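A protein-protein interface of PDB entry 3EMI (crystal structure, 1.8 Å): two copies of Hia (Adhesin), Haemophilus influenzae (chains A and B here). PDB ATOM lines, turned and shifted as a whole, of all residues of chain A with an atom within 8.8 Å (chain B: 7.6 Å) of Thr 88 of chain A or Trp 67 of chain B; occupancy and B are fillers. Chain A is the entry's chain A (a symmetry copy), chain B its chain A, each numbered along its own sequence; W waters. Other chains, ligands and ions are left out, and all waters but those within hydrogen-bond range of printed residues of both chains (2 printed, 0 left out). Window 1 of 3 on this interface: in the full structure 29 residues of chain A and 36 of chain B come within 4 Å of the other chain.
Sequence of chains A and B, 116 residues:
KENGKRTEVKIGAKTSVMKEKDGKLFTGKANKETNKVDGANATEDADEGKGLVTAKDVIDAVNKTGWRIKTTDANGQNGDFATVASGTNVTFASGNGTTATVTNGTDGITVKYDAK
Printed residues of chain A that touch a printed residue of chain B: Asn 63, Trp 67, Val 84, Ser 86, Gly 87, Thr 88, Asn 89, Val 90, Thr 91, Phe 92, Val 102, Ile 109 and Val 111. Hydrophobic or aromatic side chains of chain A within 4 Å of the printed part of chain B: Trp 67, Val 84, Val 90, Phe 92, Val 102, Ile 109 and Val 111. Among the printed residues, 27 pairs touch across the chains. Among the printed residues, no Asp or Glu carboxylate lies within 4 Å of a Lys or Arg side-chain nitrogen of the other chain.
Thr 88 of chain A touches Trp 67 of chain B, but with the chains exchanged Trp 67 of chain A does not touch Thr 88 of chain B (9.7 Å). Positions printed for both chains: 64, 65, 66, 67, 69, 82, 83, 84, 85, 86, 88, 90 and 92.
Printed residues of chain B within 4 Å of Trp 67 of chain A: Trp 67 (3.2 Å). Of the printed residues of chain B, Thr 91 of chain A touches Lys 70 (3.8 Å). Of the printed residues of chain A, Gly 23 of chain B touches Ser 86 (3.2 Å) and Gly 87 (3.7 Å). Trp 67 of chain B touches just these residues of chain A: Trp 67 (3.2 Å), Val 84 (3.6 Å), Thr 88 (3.6 Å) and Val 90 (3.4 Å). No residue of chain A comes within 4 Å of Val 84 of chain B. The nearest residue of chain A that does not touch Trp 67 of chain B is Gly 87 of chain A (4.2 Å).
The indole nitrogen (NE1) of Trp 67 of chain A sits close to the indole nitrogen (NE1) of Trp 67 of chain B, 3.4 Å away. The backbone carbonyl oxygen (O) of Gly 66 of chain B lies within hydrogen-bond range of the backbone NH (N) of Gly 87 of chain A, 2.8 Å away. The backbone NH of Val 90 of chain A lies within hydrogen-bond range of the backbone carbonyl oxygen of Arg 68 of chain B (2.7 Å). The backbone NH of Lys 70 of chain B sits at hydrogen-bond distance from the backbone carbonyl oxygen of Val 90 of chain A, 3.0 Å away. N of Arg 68 of chain B is in hydrogen-bond range of O of Thr 88 of chain A (2.8 Å).
The backbone carbonyl oxygen (O) of Trp 67 of chain B sits at hydrogen-bond distance from the backbone NH (N) of Val 84 of chain B. The backbone NH (N) of Ile 69 of chain B lies within hydrogen-bond range of the backbone carbonyl oxygen (O) of Ala 82 of chain B (2.8 Å).
Water W2 bridges the backbone NH of Phe 92 of chain A and the backbone carbonyl oxygen of Lys 70 of chain B. Water W1 bridges the side-chain amide oxygen of Asn 89 of chain A (2.8 Å) and the guanidinium group of Arg 68 of chain B (2.8 Å).
Among the printed residues, merely in contact across the chains: Asn 63 of chain A with Lys 24 of chain B (3.4 Å), Val 84 of chain A with Trp 67 of chain B (3.6 Å), Ser 86 of chain A with Gly 23 of chain B (3.2 Å), Ser 86 of chain A with Gly 66 of chain B (3.5 Å), Gly 87 of chain A with Asp 22 of chain B (3.5 Å), Gly 87 of chain A with Gly 23 of chain B (3.7 Å), Gly 87 of chain A with Arg 68 of chain B (3.8 Å), Thr 88 of chain A with Trp 67 of chain B (3.6 Å), Asn 89 of chain A with Arg 68 of chain B (3.2 Å), Asn 89 of chain A with Phe 81 of chain B (3.4 Å), Val 90 of chain A with Trp 67 of chain B (3.4 Å), Val 90 of chain A with Ile 69 of chain B (3.4 Å), Val 90 of chain A with Phe 81 of chain B (3.9 Å), Thr 91 of chain A with Lys 70 of chain B (3.8 Å), Phe 92 of chain A with Ile 69 of chain B (3.6 Å), Phe 92 of chain A with Phe 92 of chain B (3.6 Å), Val 102 of chain A with Ile 69 of chain B (3.7 Å), Val 102 of chain A with Lys 70 of chain B (3.3 Å), Ile 109 of chain A with Ile 69 of chain B (3.95 Å), Ile 109 of chain A with Val 90 of chain B (3.4 Å), Val 111 of chain A with Ile 69 of chain B (3.9 Å) and Val 111 of chain A with Phe 92 of chain B (3.5 Å).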
ATOM      1  N   ASN A  63     -16.691 -39.337  -8.651  1.00  0.00           N
ATOM      2  CA  ASN A  63     -17.453 -38.354  -9.418  1.00  0.00           C
ATOM      3  C   ASN A  63     -18.791 -37.993  -8.773  1.00  0.00           C
ATOM      4  O   ASN A  63     -19.329 -36.911  -9.007  1.00  0.00           O
ATOM      5  CB  ASN A  63     -17.661 -38.837 -10.850  1.00  0.00           C
ATOM      6  CG  ASN A  63     -16.420 -38.667 -11.699  1.00  0.00           C
ATOM      7  OD1 ASN A  63     -15.466 -38.003 -11.289  1.00  0.00           O
ATOM      8  ND2 ASN A  63     -16.425 -39.260 -12.888  1.00  0.00           N
ATOM      9  N   LYS A  64     -19.327 -38.899  -7.966  1.00  0.00           N
ATOM     10  CA  LYS A  64     -20.601 -38.651  -7.299  1.00  0.00           C
ATOM     11  C   LYS A  64     -20.446 -37.762  -6.072  1.00  0.00           C
ATOM     12  O   LYS A  64     -21.417 -37.166  -5.614  1.00  0.00           O
ATOM     13  CB  LYS A  64     -21.245 -39.964  -6.870  1.00  0.00           C
ATOM     14  CG  LYS A  64     -21.817 -40.791  -8.003  1.00  0.00           C
ATOM     15  CD  LYS A  64     -22.264 -42.152  -7.493  1.00  0.00           C
ATOM     16  CE  LYS A  64     -22.074 -43.216  -8.560  1.00  0.00           C
ATOM     17  NZ  LYS A  64     -22.434 -44.584  -8.077  1.00  0.00           N
ATOM     18  N   THR A  65     -19.241 -37.688  -5.519  1.00  0.00           N
ATOM     19  CA  THR A  65     -19.052 -36.989  -4.251  1.00  0.00           C
ATOM     20  C   THR A  65     -18.949 -35.484  -4.449  1.00  0.00           C
ATOM     21  O   THR A  65     -18.601 -34.998  -5.526  1.00  0.00           O
ATOM     22  CB  THR A  65     -17.794 -37.455  -3.513  1.00  0.00           C
ATOM     23  OG1 THR A  65     -16.634 -37.001  -4.222  1.00  0.00           O
ATOM     24  CG2 THR A  65     -17.770 -38.983  -3.384  1.00  0.00           C
ATOM     25  N   GLY A  66     -19.234 -34.750  -3.385  1.00  0.00           N
ATOM     26  CA  GLY A  66     -19.122 -33.310  -3.431  1.00  0.00           C
ATOM     27  C   GLY A  66     -19.759 -32.674  -2.223  1.00  0.00           C
ATOM     28  O   GLY A  66     -20.237 -33.360  -1.317  1.00  0.00           O
ATOM     29  N   TRP A  67     -19.765 -31.351  -2.197  1.00  0.00           N
ATOM     30  CA  TRP A  67     -20.396 -30.672  -1.082  1.00  0.00           C
ATOM     31  C   TRP A  67     -21.861 -30.448  -1.424  1.00  0.00           C
ATOM     32  O   TRP A  67     -22.287 -30.718  -2.550  1.00  0.00           O
ATOM     33  CB  TRP A  67     -19.663 -29.374  -0.739  1.00  0.00           C
ATOM     34  CG  TRP A  67     -19.367 -28.494  -1.912  1.00  0.00           C
ATOM     35  CD1 TRP A  67     -18.510 -28.757  -2.951  1.00  0.00           C
ATOM     36  CD2 TRP A  67     -19.905 -27.190  -2.150  1.00  0.00           C
ATOM     37  NE1 TRP A  67     -18.503 -27.693  -3.829  1.00  0.00           N
ATOM     38  CE2 TRP A  67     -19.346 -26.725  -3.359  1.00  0.00           C
ATOM     39  CE3 TRP A  67     -20.811 -26.374  -1.463  1.00  0.00           C
ATOM     40  CZ2 TRP A  67     -19.661 -25.470  -3.886  1.00  0.00           C
ATOM     41  CZ3 TRP A  67     -21.123 -25.136  -1.993  1.00  0.00           C
ATOM     42  CH2 TRP A  67     -20.546 -24.695  -3.193  1.00  0.00           C
ATOM     43  N   ILE A  69     -25.080 -27.829  -1.547  1.00  0.00           N
ATOM     44  CA  ILE A  69     -25.409 -26.404  -1.522  1.00  0.00           C
ATOM     45  C   ILE A  69     -26.914 -26.194  -1.398  1.00  0.00           C
ATOM     46  O   ILE A  69     -27.704 -26.844  -2.082  1.00  0.00           O
ATOM     47  CB  ILE A  69     -24.821 -25.639  -2.736  1.00  0.00           C
ATOM     48  CG1 ILE A  69     -24.898 -24.120  -2.507  1.00  0.00           C
ATOM     49  CG2 ILE A  69     -25.515 -26.047  -4.041  1.00  0.00           C
ATOM     50  CD1 ILE A  69     -24.233 -23.319  -3.598  1.00  0.00           C
ATOM     51  N   ALA A  82     -28.437 -29.379  -3.129  1.00  0.00           N
ATOM     52  CA  ALA A  82     -28.002 -30.048  -4.341  1.00  0.00           C
ATOM     53  C   ALA A  82     -26.543 -30.417  -4.163  1.00  0.00           C
ATOM     54  O   ALA A  82     -25.785 -29.700  -3.506  1.00  0.00           O
ATOM     55  CB  ALA A  82     -28.191 -29.146  -5.546  1.00  0.00           C
ATOM     56  N   THR A  83     -26.144 -31.544  -4.727  1.00  0.00           N
ATOM     57  CA  THR A  83     -24.758 -31.956  -4.622  1.00  0.00           C
ATOM     58  C   THR A  83     -23.926 -31.253  -5.681  1.00  0.00           C
ATOM     59  O   THR A  83     -24.227 -31.322  -6.883  1.00  0.00           O
ATOM     60  CB  THR A  83     -24.600 -33.481  -4.761  1.00  0.00           C
ATOM     61  OG1 THR A  83     -25.370 -34.130  -3.746  1.00  0.00           O
ATOM     62  CG2 THR A  83     -23.141 -33.887  -4.616  1.00  0.00           C
ATOM     63  N   VAL A  84     -22.894 -30.556  -5.221  1.00  0.00           N
ATOM     64  CA  VAL A  84     -21.929 -29.933  -6.113  1.00  0.00           C
ATOM     65  C   VAL A  84     -20.838 -30.960  -6.342  1.00  0.00           C
ATOM     66  O   VAL A  84     -19.817 -30.981  -5.656  1.00  0.00           O
ATOM     67  CB  VAL A  84     -21.350 -28.653  -5.503  1.00  0.00           C
ATOM     68  CG1 VAL A  84     -20.421 -27.971  -6.485  1.00  0.00           C
ATOM     69  CG2 VAL A  84     -22.493 -27.722  -5.117  1.00  0.00           C
ATOM     70  N   ALA A  85     -21.099 -31.845  -7.295  1.00  0.00           N
ATOM     71  CA  ALA A  85     -20.244 -32.995  -7.546  1.00  0.00           C
ATOM     72  C   ALA A  85     -18.997 -32.622  -8.346  1.00  0.00           C
ATOM     73  O   ALA A  85     -18.907 -31.529  -8.903  1.00  0.00           O
ATOM     74  CB  ALA A  85     -21.036 -34.063  -8.273  1.00  0.00           C
ATOM     75  N   SER A  86     -18.038 -33.542  -8.401  1.00  0.00           N
ATOM     76  CA  SER A  86     -16.809 -33.331  -9.158  1.00  0.00           C
ATOM     77  C   SER A  86     -17.126 -32.836 -10.564  1.00  0.00           C
ATOM     78  O   SER A  86     -17.898 -33.464 -11.287  1.00  0.00           O
ATOM     79  CB  SER A  86     -16.005 -34.633  -9.226  1.00  0.00           C
ATOM     80  OG  SER A  86     -15.865 -35.199  -7.934  1.00  0.00           O
ATOM     81  N   GLY A  87     -16.549 -31.698 -10.941  1.00  0.00           N
ATOM     82  CA  GLY A  87     -16.754 -31.152 -12.269  1.00  0.00           C
ATOM     83  C   GLY A  87     -17.937 -30.203 -12.402  1.00  0.00           C
ATOM     84  O   GLY A  87     -18.126 -29.600 -13.461  1.00  0.00           O
ATOM     85  N   THR A  88     -18.736 -30.082 -11.345  1.00  0.00           N
ATOM     86  CA  THR A  88     -19.929 -29.225 -11.377  1.00  0.00           C
ATOM     87  C   THR A  88     -19.512 -27.762 -11.435  1.00  0.00           C
ATOM     88  O   THR A  88     -18.657 -27.324 -10.663  1.00  0.00           O
ATOM     89  CB  THR A  88     -20.847 -29.427 -10.141  1.00  0.00           C
ATOM     90  OG1 THR A  88     -21.362 -30.761 -10.117  1.00  0.00           O
ATOM     91  CG2 THR A  88     -22.030 -28.466 -10.191  1.00  0.00           C
ATOM     92  N   ASN A  89     -20.112 -27.017 -12.360  1.00  0.00           N
ATOM     93  CA  ASN A  89     -19.822 -25.595 -12.532  1.00  0.00           C
ATOM     94  C   ASN A  89     -20.573 -24.757 -11.513  1.00  0.00           C
ATOM     95  O   ASN A  89     -21.756 -24.984 -11.269  1.00  0.00           O
ATOM     96  CB  ASN A  89     -20.216 -25.142 -13.942  1.00  0.00           C
ATOM     97  CG  ASN A  89     -19.212 -25.557 -14.990  1.00  0.00           C
ATOM     98  OD1 ASN A  89     -18.186 -26.160 -14.679  1.00  0.00           O
ATOM     99  ND2 ASN A  89     -19.500 -25.232 -16.249  1.00  0.00           N
ATOM    100  N   VAL A  90     -19.881 -23.787 -10.926  1.00  0.00           N
ATOM    101  CA  VAL A  90     -20.486 -22.883  -9.965  1.00  0.00           C
ATOM    102  C   VAL A  90     -20.123 -21.458 -10.357  1.00  0.00           C
ATOM    103  O   VAL A  90     -18.952 -21.149 -10.581  1.00  0.00           O
ATOM    104  CB  VAL A  90     -20.013 -23.178  -8.534  1.00  0.00           C
ATOM    105  CG1 VAL A  90     -20.639 -22.193  -7.546  1.00  0.00           C
ATOM    106  CG2 VAL A  90     -20.354 -24.621  -8.149  1.00  0.00           C
ATOM    107  N   THR A  91     -21.141 -20.611 -10.459  1.00  0.00           N
ATOM    108  CA  THR A  91     -20.956 -19.223 -10.850  1.00  0.00           C
ATOM    109  C   THR A  91     -21.456 -18.310  -9.744  1.00  0.00           C
ATOM    110  O   THR A  91     -22.556 -18.501  -9.217  1.00  0.00           O
ATOM    111  CB  THR A  91     -21.743 -18.921 -12.144  1.00  0.00           C
ATOM    112  OG1 THR A  91     -21.257 -19.747 -13.206  1.00  0.00           O
ATOM    113  CG2 THR A  91     -21.621 -17.453 -12.553  1.00  0.00           C
ATOM    114  N   PHE A  92     -20.634 -17.338  -9.366  1.00  0.00           N
ATOM    115  CA  PHE A  92     -21.081 -16.304  -8.444  1.00  0.00           C
ATOM    116  C   PHE A  92     -21.449 -15.065  -9.252  1.00  0.00           C
ATOM    117  O   PHE A  92     -20.583 -14.312  -9.684  1.00  0.00           O
ATOM    118  CB  PHE A  92     -20.022 -16.042  -7.372  1.00  0.00           C
ATOM    119  CG  PHE A  92     -19.859 -17.190  -6.427  1.00  0.00           C
ATOM    120  CD1 PHE A  92     -20.594 -17.244  -5.254  1.00  0.00           C
ATOM    121  CD2 PHE A  92     -19.027 -18.253  -6.745  1.00  0.00           C
ATOM    122  CE1 PHE A  92     -20.478 -18.325  -4.400  1.00  0.00           C
ATOM    123  CE2 PHE A  92     -18.907 -19.337  -5.889  1.00  0.00           C
ATOM    124  CZ  PHE A  92     -19.633 -19.370  -4.717  1.00  0.00           C
ATOM    125  N   VAL A 102     -14.361 -13.016  -9.033  1.00  0.00           N
ATOM    126  CA  VAL A 102     -13.772 -14.253  -8.544  1.00  0.00           C
ATOM    127  C   VAL A 102     -12.359 -14.338  -9.085  1.00  0.00           C
ATOM    128  O   VAL A 102     -12.160 -14.413 -10.291  1.00  0.00           O
ATOM    129  CB  VAL A 102     -14.562 -15.493  -9.003  1.00  0.00           C
ATOM    130  CG1 VAL A 102     -13.884 -16.752  -8.501  1.00  0.00           C
ATOM    131  CG2 VAL A 102     -16.012 -15.432  -8.512  1.00  0.00           C
ATOM    132  N   ILE A 109      -8.579 -19.176  -4.144  1.00  0.00           N
ATOM    133  CA  ILE A 109      -9.674 -18.479  -4.790  1.00  0.00           C
ATOM    134  C   ILE A 109     -10.262 -17.436  -3.860  1.00  0.00           C
ATOM    135  O   ILE A 109     -10.431 -17.683  -2.667  1.00  0.00           O
ATOM    136  CB  ILE A 109     -10.798 -19.462  -5.143  1.00  0.00           C
ATOM    137  CG1 ILE A 109     -10.271 -20.555  -6.077  1.00  0.00           C
ATOM    138  CG2 ILE A 109     -11.976 -18.721  -5.756  1.00  0.00           C
ATOM    139  CD1 ILE A 109      -9.673 -20.018  -7.345  1.00  0.00           C
ATOM    140  N   VAL A 111     -13.637 -14.974  -3.673  1.00  0.00           N
ATOM    141  CA  VAL A 111     -14.909 -14.480  -4.165  1.00  0.00           C
ATOM    142  C   VAL A 111     -15.195 -13.183  -3.418  1.00  0.00           C
ATOM    143  O   VAL A 111     -14.916 -13.063  -2.223  1.00  0.00           O
ATOM    144  CB  VAL A 111     -16.047 -15.479  -3.880  1.00  0.00           C
ATOM    145  CG1 VAL A 111     -17.398 -14.889  -4.277  1.00  0.00           C
ATOM    146  CG2 VAL A 111     -15.800 -16.797  -4.602  1.00  0.00           C
ATOM    147  N   ASP B  22     -10.948 -31.244 -15.881  1.00  0.00           N
ATOM    148  CA  ASP B  22     -11.829 -30.220 -15.337  1.00  0.00           C
ATOM    149  C   ASP B  22     -12.503 -30.659 -14.041  1.00  0.00           C
ATOM    150  O   ASP B  22     -13.670 -30.341 -13.809  1.00  0.00           O
ATOM    151  CB  ASP B  22     -12.893 -29.827 -16.360  1.00  0.00           C
ATOM    152  CG  ASP B  22     -12.306 -29.172 -17.591  1.00  0.00           C
ATOM    153  OD1 ASP B  22     -11.110 -28.807 -17.570  1.00  0.00           O
ATOM    154  OD2 ASP B  22     -13.056 -29.011 -18.578  1.00  0.00           O
ATOM    155  N   GLY B  23     -11.768 -31.391 -13.209  1.00  0.00           N
ATOM    156  CA  GLY B  23     -12.221 -31.706 -11.864  1.00  0.00           C
ATOM    157  C   GLY B  23     -12.942 -33.036 -11.743  1.00  0.00           C
ATOM    158  O   GLY B  23     -13.348 -33.437 -10.650  1.00  0.00           O
ATOM    159  N   LYS B  24     -13.104 -33.711 -12.875  1.00  0.00           N
ATOM    160  CA  LYS B  24     -13.860 -34.952 -12.943  1.00  0.00           C
ATOM    161  C   LYS B  24     -12.957 -36.070 -13.438  1.00  0.00           C
ATOM    162  O   LYS B  24     -12.037 -35.834 -14.225  1.00  0.00           O
ATOM    163  CB  LYS B  24     -15.050 -34.775 -13.894  1.00  0.00           C
ATOM    164  CG  LYS B  24     -16.053 -35.910 -13.874  1.00  0.00           C
ATOM    165  CD  LYS B  24     -17.272 -35.549 -14.718  1.00  0.00           C
ATOM    166  CE  LYS B  24     -18.154 -36.762 -14.983  1.00  0.00           C
ATOM    167  NZ  LYS B  24     -19.358 -36.377 -15.760  1.00  0.00           N
ATOM    168  N   LYS B  64      -6.942 -34.321  -7.700  1.00  0.00           N
ATOM    169  CA  LYS B  64      -7.206 -33.530  -8.897  1.00  0.00           C
ATOM    170  C   LYS B  64      -8.670 -33.123  -9.009  1.00  0.00           C
ATOM    171  O   LYS B  64      -8.996 -32.182  -9.727  1.00  0.00           O
ATOM    172  CB  LYS B  64      -6.824 -34.312 -10.150  1.00  0.00           C
ATOM    173  CG  LYS B  64      -5.332 -34.453 -10.378  1.00  0.00           C
ATOM    174  CD  LYS B  64      -5.062 -35.398 -11.539  1.00  0.00           C
ATOM    175  CE  LYS B  64      -3.772 -36.169 -11.316  1.00  0.00           C
ATOM    176  NZ  LYS B  64      -3.503 -37.162 -12.400  1.00  0.00           N
ATOM    177  N   THR B  65      -9.557 -33.838  -8.325  1.00  0.00           N
ATOM    178  CA  THR B  65     -10.987 -33.610  -8.510  1.00  0.00           C
ATOM    179  C   THR B  65     -11.474 -32.415  -7.705  1.00  0.00           C
ATOM    180  O   THR B  65     -10.867 -32.019  -6.708  1.00  0.00           O
ATOM    181  CB  THR B  65     -11.826 -34.826  -8.103  1.00  0.00           C
ATOM    182  OG1 THR B  65     -11.779 -34.976  -6.678  1.00  0.00           O
ATOM    183  CG2 THR B  65     -11.310 -36.098  -8.787  1.00  0.00           C
ATOM    184  N   GLY B  66     -12.594 -31.856  -8.137  1.00  0.00           N
ATOM    185  CA  GLY B  66     -13.186 -30.746  -7.426  1.00  0.00           C
ATOM    186  C   GLY B  66     -14.276 -30.097  -8.239  1.00  0.00           C
ATOM    187  O   GLY B  66     -14.612 -30.550  -9.335  1.00  0.00           O
ATOM    188  N   TRP B  67     -14.843 -29.028  -7.705  1.00  0.00           N
ATOM    189  CA  TRP B  67     -15.873 -28.330  -8.448  1.00  0.00           C
ATOM    190  C   TRP B  67     -15.206 -27.269  -9.308  1.00  0.00           C
ATOM    191  O   TRP B  67     -13.998 -27.042  -9.197  1.00  0.00           O
ATOM    192  CB  TRP B  67     -16.936 -27.753  -7.513  1.00  0.00           C
ATOM    193  CG  TRP B  67     -16.395 -26.992  -6.345  1.00  0.00           C
ATOM    194  CD1 TRP B  67     -15.674 -27.494  -5.289  1.00  0.00           C
ATOM    195  CD2 TRP B  67     -16.560 -25.593  -6.095  1.00  0.00           C
ATOM    196  NE1 TRP B  67     -15.368 -26.476  -4.410  1.00  0.00           N
ATOM    197  CE2 TRP B  67     -15.900 -25.308  -4.881  1.00  0.00           C
ATOM    198  CE3 TRP B  67     -17.193 -24.553  -6.783  1.00  0.00           C
ATOM    199  CZ2 TRP B  67     -15.869 -24.020  -4.339  1.00  0.00           C
ATOM    200  CZ3 TRP B  67     -17.154 -23.279  -6.246  1.00  0.00           C
ATOM    201  CH2 TRP B  67     -16.498 -23.026  -5.032  1.00  0.00           C
ATOM    202  N   ARG B  68     -15.979 -26.643 -10.186  1.00  0.00           N
ATOM    203  CA  ARG B  68     -15.417 -25.688 -11.130  1.00  0.00           C
ATOM    204  C   ARG B  68     -16.009 -24.328 -10.815  1.00  0.00           C
ATOM    205  O   ARG B  68     -17.223 -24.197 -10.709  1.00  0.00           O
ATOM    206  CB  ARG B  68     -15.739 -26.105 -12.572  1.00  0.00           C
ATOM    207  CG  ARG B  68     -15.037 -27.391 -12.998  1.00  0.00           C
ATOM    208  CD  ARG B  68     -13.593 -27.104 -13.407  1.00  0.00           C
ATOM    209  NE  ARG B  68     -13.521 -26.525 -14.744  1.00  0.00           N
ATOM    210  CZ  ARG B  68     -12.394 -26.160 -15.343  1.00  0.00           C
ATOM    211  NH1 ARG B  68     -11.227 -26.305 -14.724  1.00  0.00           N
ATOM    212  NH2 ARG B  68     -12.432 -25.642 -16.562  1.00  0.00           N
ATOM    213  N   ILE B  69     -15.157 -23.328 -10.617  1.00  0.00           N
ATOM    214  CA  ILE B  69     -15.663 -21.997 -10.285  1.00  0.00           C
ATOM    215  C   ILE B  69     -15.375 -21.008 -11.411  1.00  0.00           C
ATOM    216  O   ILE B  69     -14.270 -20.967 -11.952  1.00  0.00           O
ATOM    217  CB  ILE B  69     -15.132 -21.484  -8.922  1.00  0.00           C
ATOM    218  CG1 ILE B  69     -15.931 -20.254  -8.457  1.00  0.00           C
ATOM    219  CG2 ILE B  69     -13.628 -21.187  -8.985  1.00  0.00           C
ATOM    220  CD1 ILE B  69     -15.545 -19.778  -7.081  1.00  0.00           C
ATOM    221  N   LYS B  70     -16.384 -20.232 -11.782  1.00  0.00           N
ATOM    222  CA  LYS B  70     -16.207 -19.252 -12.844  1.00  0.00           C
ATOM    223  C   LYS B  70     -15.381 -18.085 -12.313  1.00  0.00           C
ATOM    224  O   LYS B  70     -15.759 -17.445 -11.336  1.00  0.00           O
ATOM    225  CB  LYS B  70     -17.560 -18.759 -13.341  1.00  0.00           C
ATOM    226  CG  LYS B  70     -17.478 -17.502 -14.170  1.00  0.00           C
ATOM    227  CD  LYS B  70     -16.989 -17.808 -15.558  1.00  0.00           C
ATOM    228  CE  LYS B  70     -17.876 -18.849 -16.204  1.00  0.00           C
ATOM    229  NZ  LYS B  70     -17.774 -18.773 -17.676  1.00  0.00           N
ATOM    230  N   PHE B  81     -13.297 -21.078 -16.171  1.00  0.00           N
ATOM    231  CA  PHE B  81     -13.502 -21.789 -14.920  1.00  0.00           C
ATOM    232  C   PHE B  81     -12.145 -22.215 -14.369  1.00  0.00           C
ATOM    233  O   PHE B  81     -11.162 -22.338 -15.111  1.00  0.00           O
ATOM    234  CB  PHE B  81     -14.386 -23.016 -15.128  1.00  0.00           C
ATOM    235  CG  PHE B  81     -15.844 -22.697 -15.239  1.00  0.00           C
ATOM    236  CD1 PHE B  81     -16.637 -22.645 -14.108  1.00  0.00           C
ATOM    237  CD2 PHE B  81     -16.426 -22.447 -16.474  1.00  0.00           C
ATOM    238  CE1 PHE B  81     -17.984 -22.355 -14.200  1.00  0.00           C
ATOM    239  CE2 PHE B  81     -17.773 -22.155 -16.576  1.00  0.00           C
ATOM    240  CZ  PHE B  81     -18.553 -22.109 -15.432  1.00  0.00           C
ATOM    241  N   ALA B  82     -12.095 -22.417 -13.060  1.00  0.00           N
ATOM    242  CA  ALA B  82     -10.924 -22.978 -12.414  1.00  0.00           C
ATOM    243  C   ALA B  82     -11.389 -24.125 -11.538  1.00  0.00           C
ATOM    244  O   ALA B  82     -12.488 -24.088 -10.980  1.00  0.00           O
ATOM    245  CB  ALA B  82     -10.209 -21.923 -11.591  1.00  0.00           C
ATOM    246  N   THR B  83     -10.569 -25.156 -11.428  1.00  0.00           N
ATOM    247  CA  THR B  83     -10.931 -26.284 -10.591  1.00  0.00           C
ATOM    248  C   THR B  83     -10.584 -25.986  -9.142  1.00  0.00           C
ATOM    249  O   THR B  83      -9.435 -25.653  -8.812  1.00  0.00           O
ATOM    250  CB  THR B  83     -10.231 -27.579 -11.039  1.00  0.00           C
ATOM    251  OG1 THR B  83     -10.583 -27.860 -12.397  1.00  0.00           O
ATOM    252  CG2 THR B  83     -10.653 -28.749 -10.163  1.00  0.00           C
ATOM    253  N   VAL B  84     -11.594 -26.082  -8.287  1.00  0.00           N
ATOM    254  CA  VAL B  84     -11.399 -25.955  -6.850  1.00  0.00           C
ATOM    255  C   VAL B  84     -11.128 -27.353  -6.333  1.00  0.00           C
ATOM    256  O   VAL B  84     -12.031 -28.066  -5.896  1.00  0.00           O
ATOM    257  CB  VAL B  84     -12.634 -25.355  -6.171  1.00  0.00           C
ATOM    258  CG1 VAL B  84     -12.375 -25.143  -4.694  1.00  0.00           C
ATOM    259  CG2 VAL B  84     -12.983 -24.033  -6.845  1.00  0.00           C
ATOM    260  N   ALA B  85      -9.866 -27.749  -6.436  1.00  0.00           N
ATOM    261  CA  ALA B  85      -9.450 -29.111  -6.140  1.00  0.00           C
ATOM    262  C   ALA B  85      -9.320 -29.359  -4.637  1.00  0.00           C
ATOM    263  O   ALA B  85      -9.326 -28.423  -3.839  1.00  0.00           O
ATOM    264  CB  ALA B  85      -8.135 -29.399  -6.837  1.00  0.00           C
ATOM    265  N   SER B  86      -9.198 -30.629  -4.261  1.00  0.00           N
ATOM    266  CA  SER B  86      -9.033 -31.007  -2.862  1.00  0.00           C
ATOM    267  C   SER B  86      -7.937 -30.172  -2.209  1.00  0.00           C
ATOM    268  O   SER B  86      -6.814 -30.116  -2.709  1.00  0.00           O
ATOM    269  CB  SER B  86      -8.693 -32.497  -2.758  1.00  0.00           C
ATOM    270  OG  SER B  86      -9.605 -33.269  -3.519  1.00  0.00           O
ATOM    271  N   THR B  88      -7.896 -26.901  -1.909  1.00  0.00           N
ATOM    272  CA  THR B  88      -7.844 -25.536  -2.448  1.00  0.00           C
ATOM    273  C   THR B  88      -8.532 -24.575  -1.488  1.00  0.00           C
ATOM    274  O   THR B  88      -9.645 -24.840  -1.030  1.00  0.00           O
ATOM    275  CB  THR B  88      -8.521 -25.412  -3.839  1.00  0.00           C
ATOM    276  OG1 THR B  88      -7.825 -26.208  -4.804  1.00  0.00           O
ATOM    277  CG2 THR B  88      -8.497 -23.965  -4.318  1.00  0.00           C
ATOM    278  N   VAL B  90     -10.493 -21.247  -0.358  1.00  0.00           N
ATOM    279  CA  VAL B  90     -11.493 -20.354  -0.914  1.00  0.00           C
ATOM    280  C   VAL B  90     -11.864 -19.333   0.151  1.00  0.00           C
ATOM    281  O   VAL B  90     -12.175 -19.695   1.286  1.00  0.00           O
ATOM    282  CB  VAL B  90     -12.742 -21.119  -1.375  1.00  0.00           C
ATOM    283  CG1 VAL B  90     -13.792 -20.154  -1.926  1.00  0.00           C
ATOM    284  CG2 VAL B  90     -12.365 -22.166  -2.428  1.00  0.00           C
ATOM    285  N   PHE B  92     -14.251 -15.896   0.998  1.00  0.00           N
ATOM    286  CA  PHE B  92     -15.322 -14.979   0.635  1.00  0.00           C
ATOM    287  C   PHE B  92     -15.028 -13.623   1.268  1.00  0.00           C
ATOM    288  O   PHE B  92     -15.247 -13.419   2.456  1.00  0.00           O
ATOM    289  CB  PHE B  92     -16.682 -15.555   1.031  1.00  0.00           C
ATOM    290  CG  PHE B  92     -17.065 -16.747   0.214  1.00  0.00           C
ATOM    291  CD1 PHE B  92     -17.808 -16.595  -0.946  1.00  0.00           C
ATOM    292  CD2 PHE B  92     -16.619 -18.014   0.562  1.00  0.00           C
ATOM    293  CE1 PHE B  92     -18.126 -17.691  -1.726  1.00  0.00           C
ATOM    294  CE2 PHE B  92     -16.940 -19.115  -0.218  1.00  0.00           C
ATOM    295  CZ  PHE B  92     -17.692 -18.950  -1.362  1.00  0.00           C
HETATM  296  O   HOH W   1     -15.906 -26.402 -16.208  1.00  0.00           O
HETATM  297  O   HOH W   2     -18.406 -16.595 -10.717  1.00  0.00           O
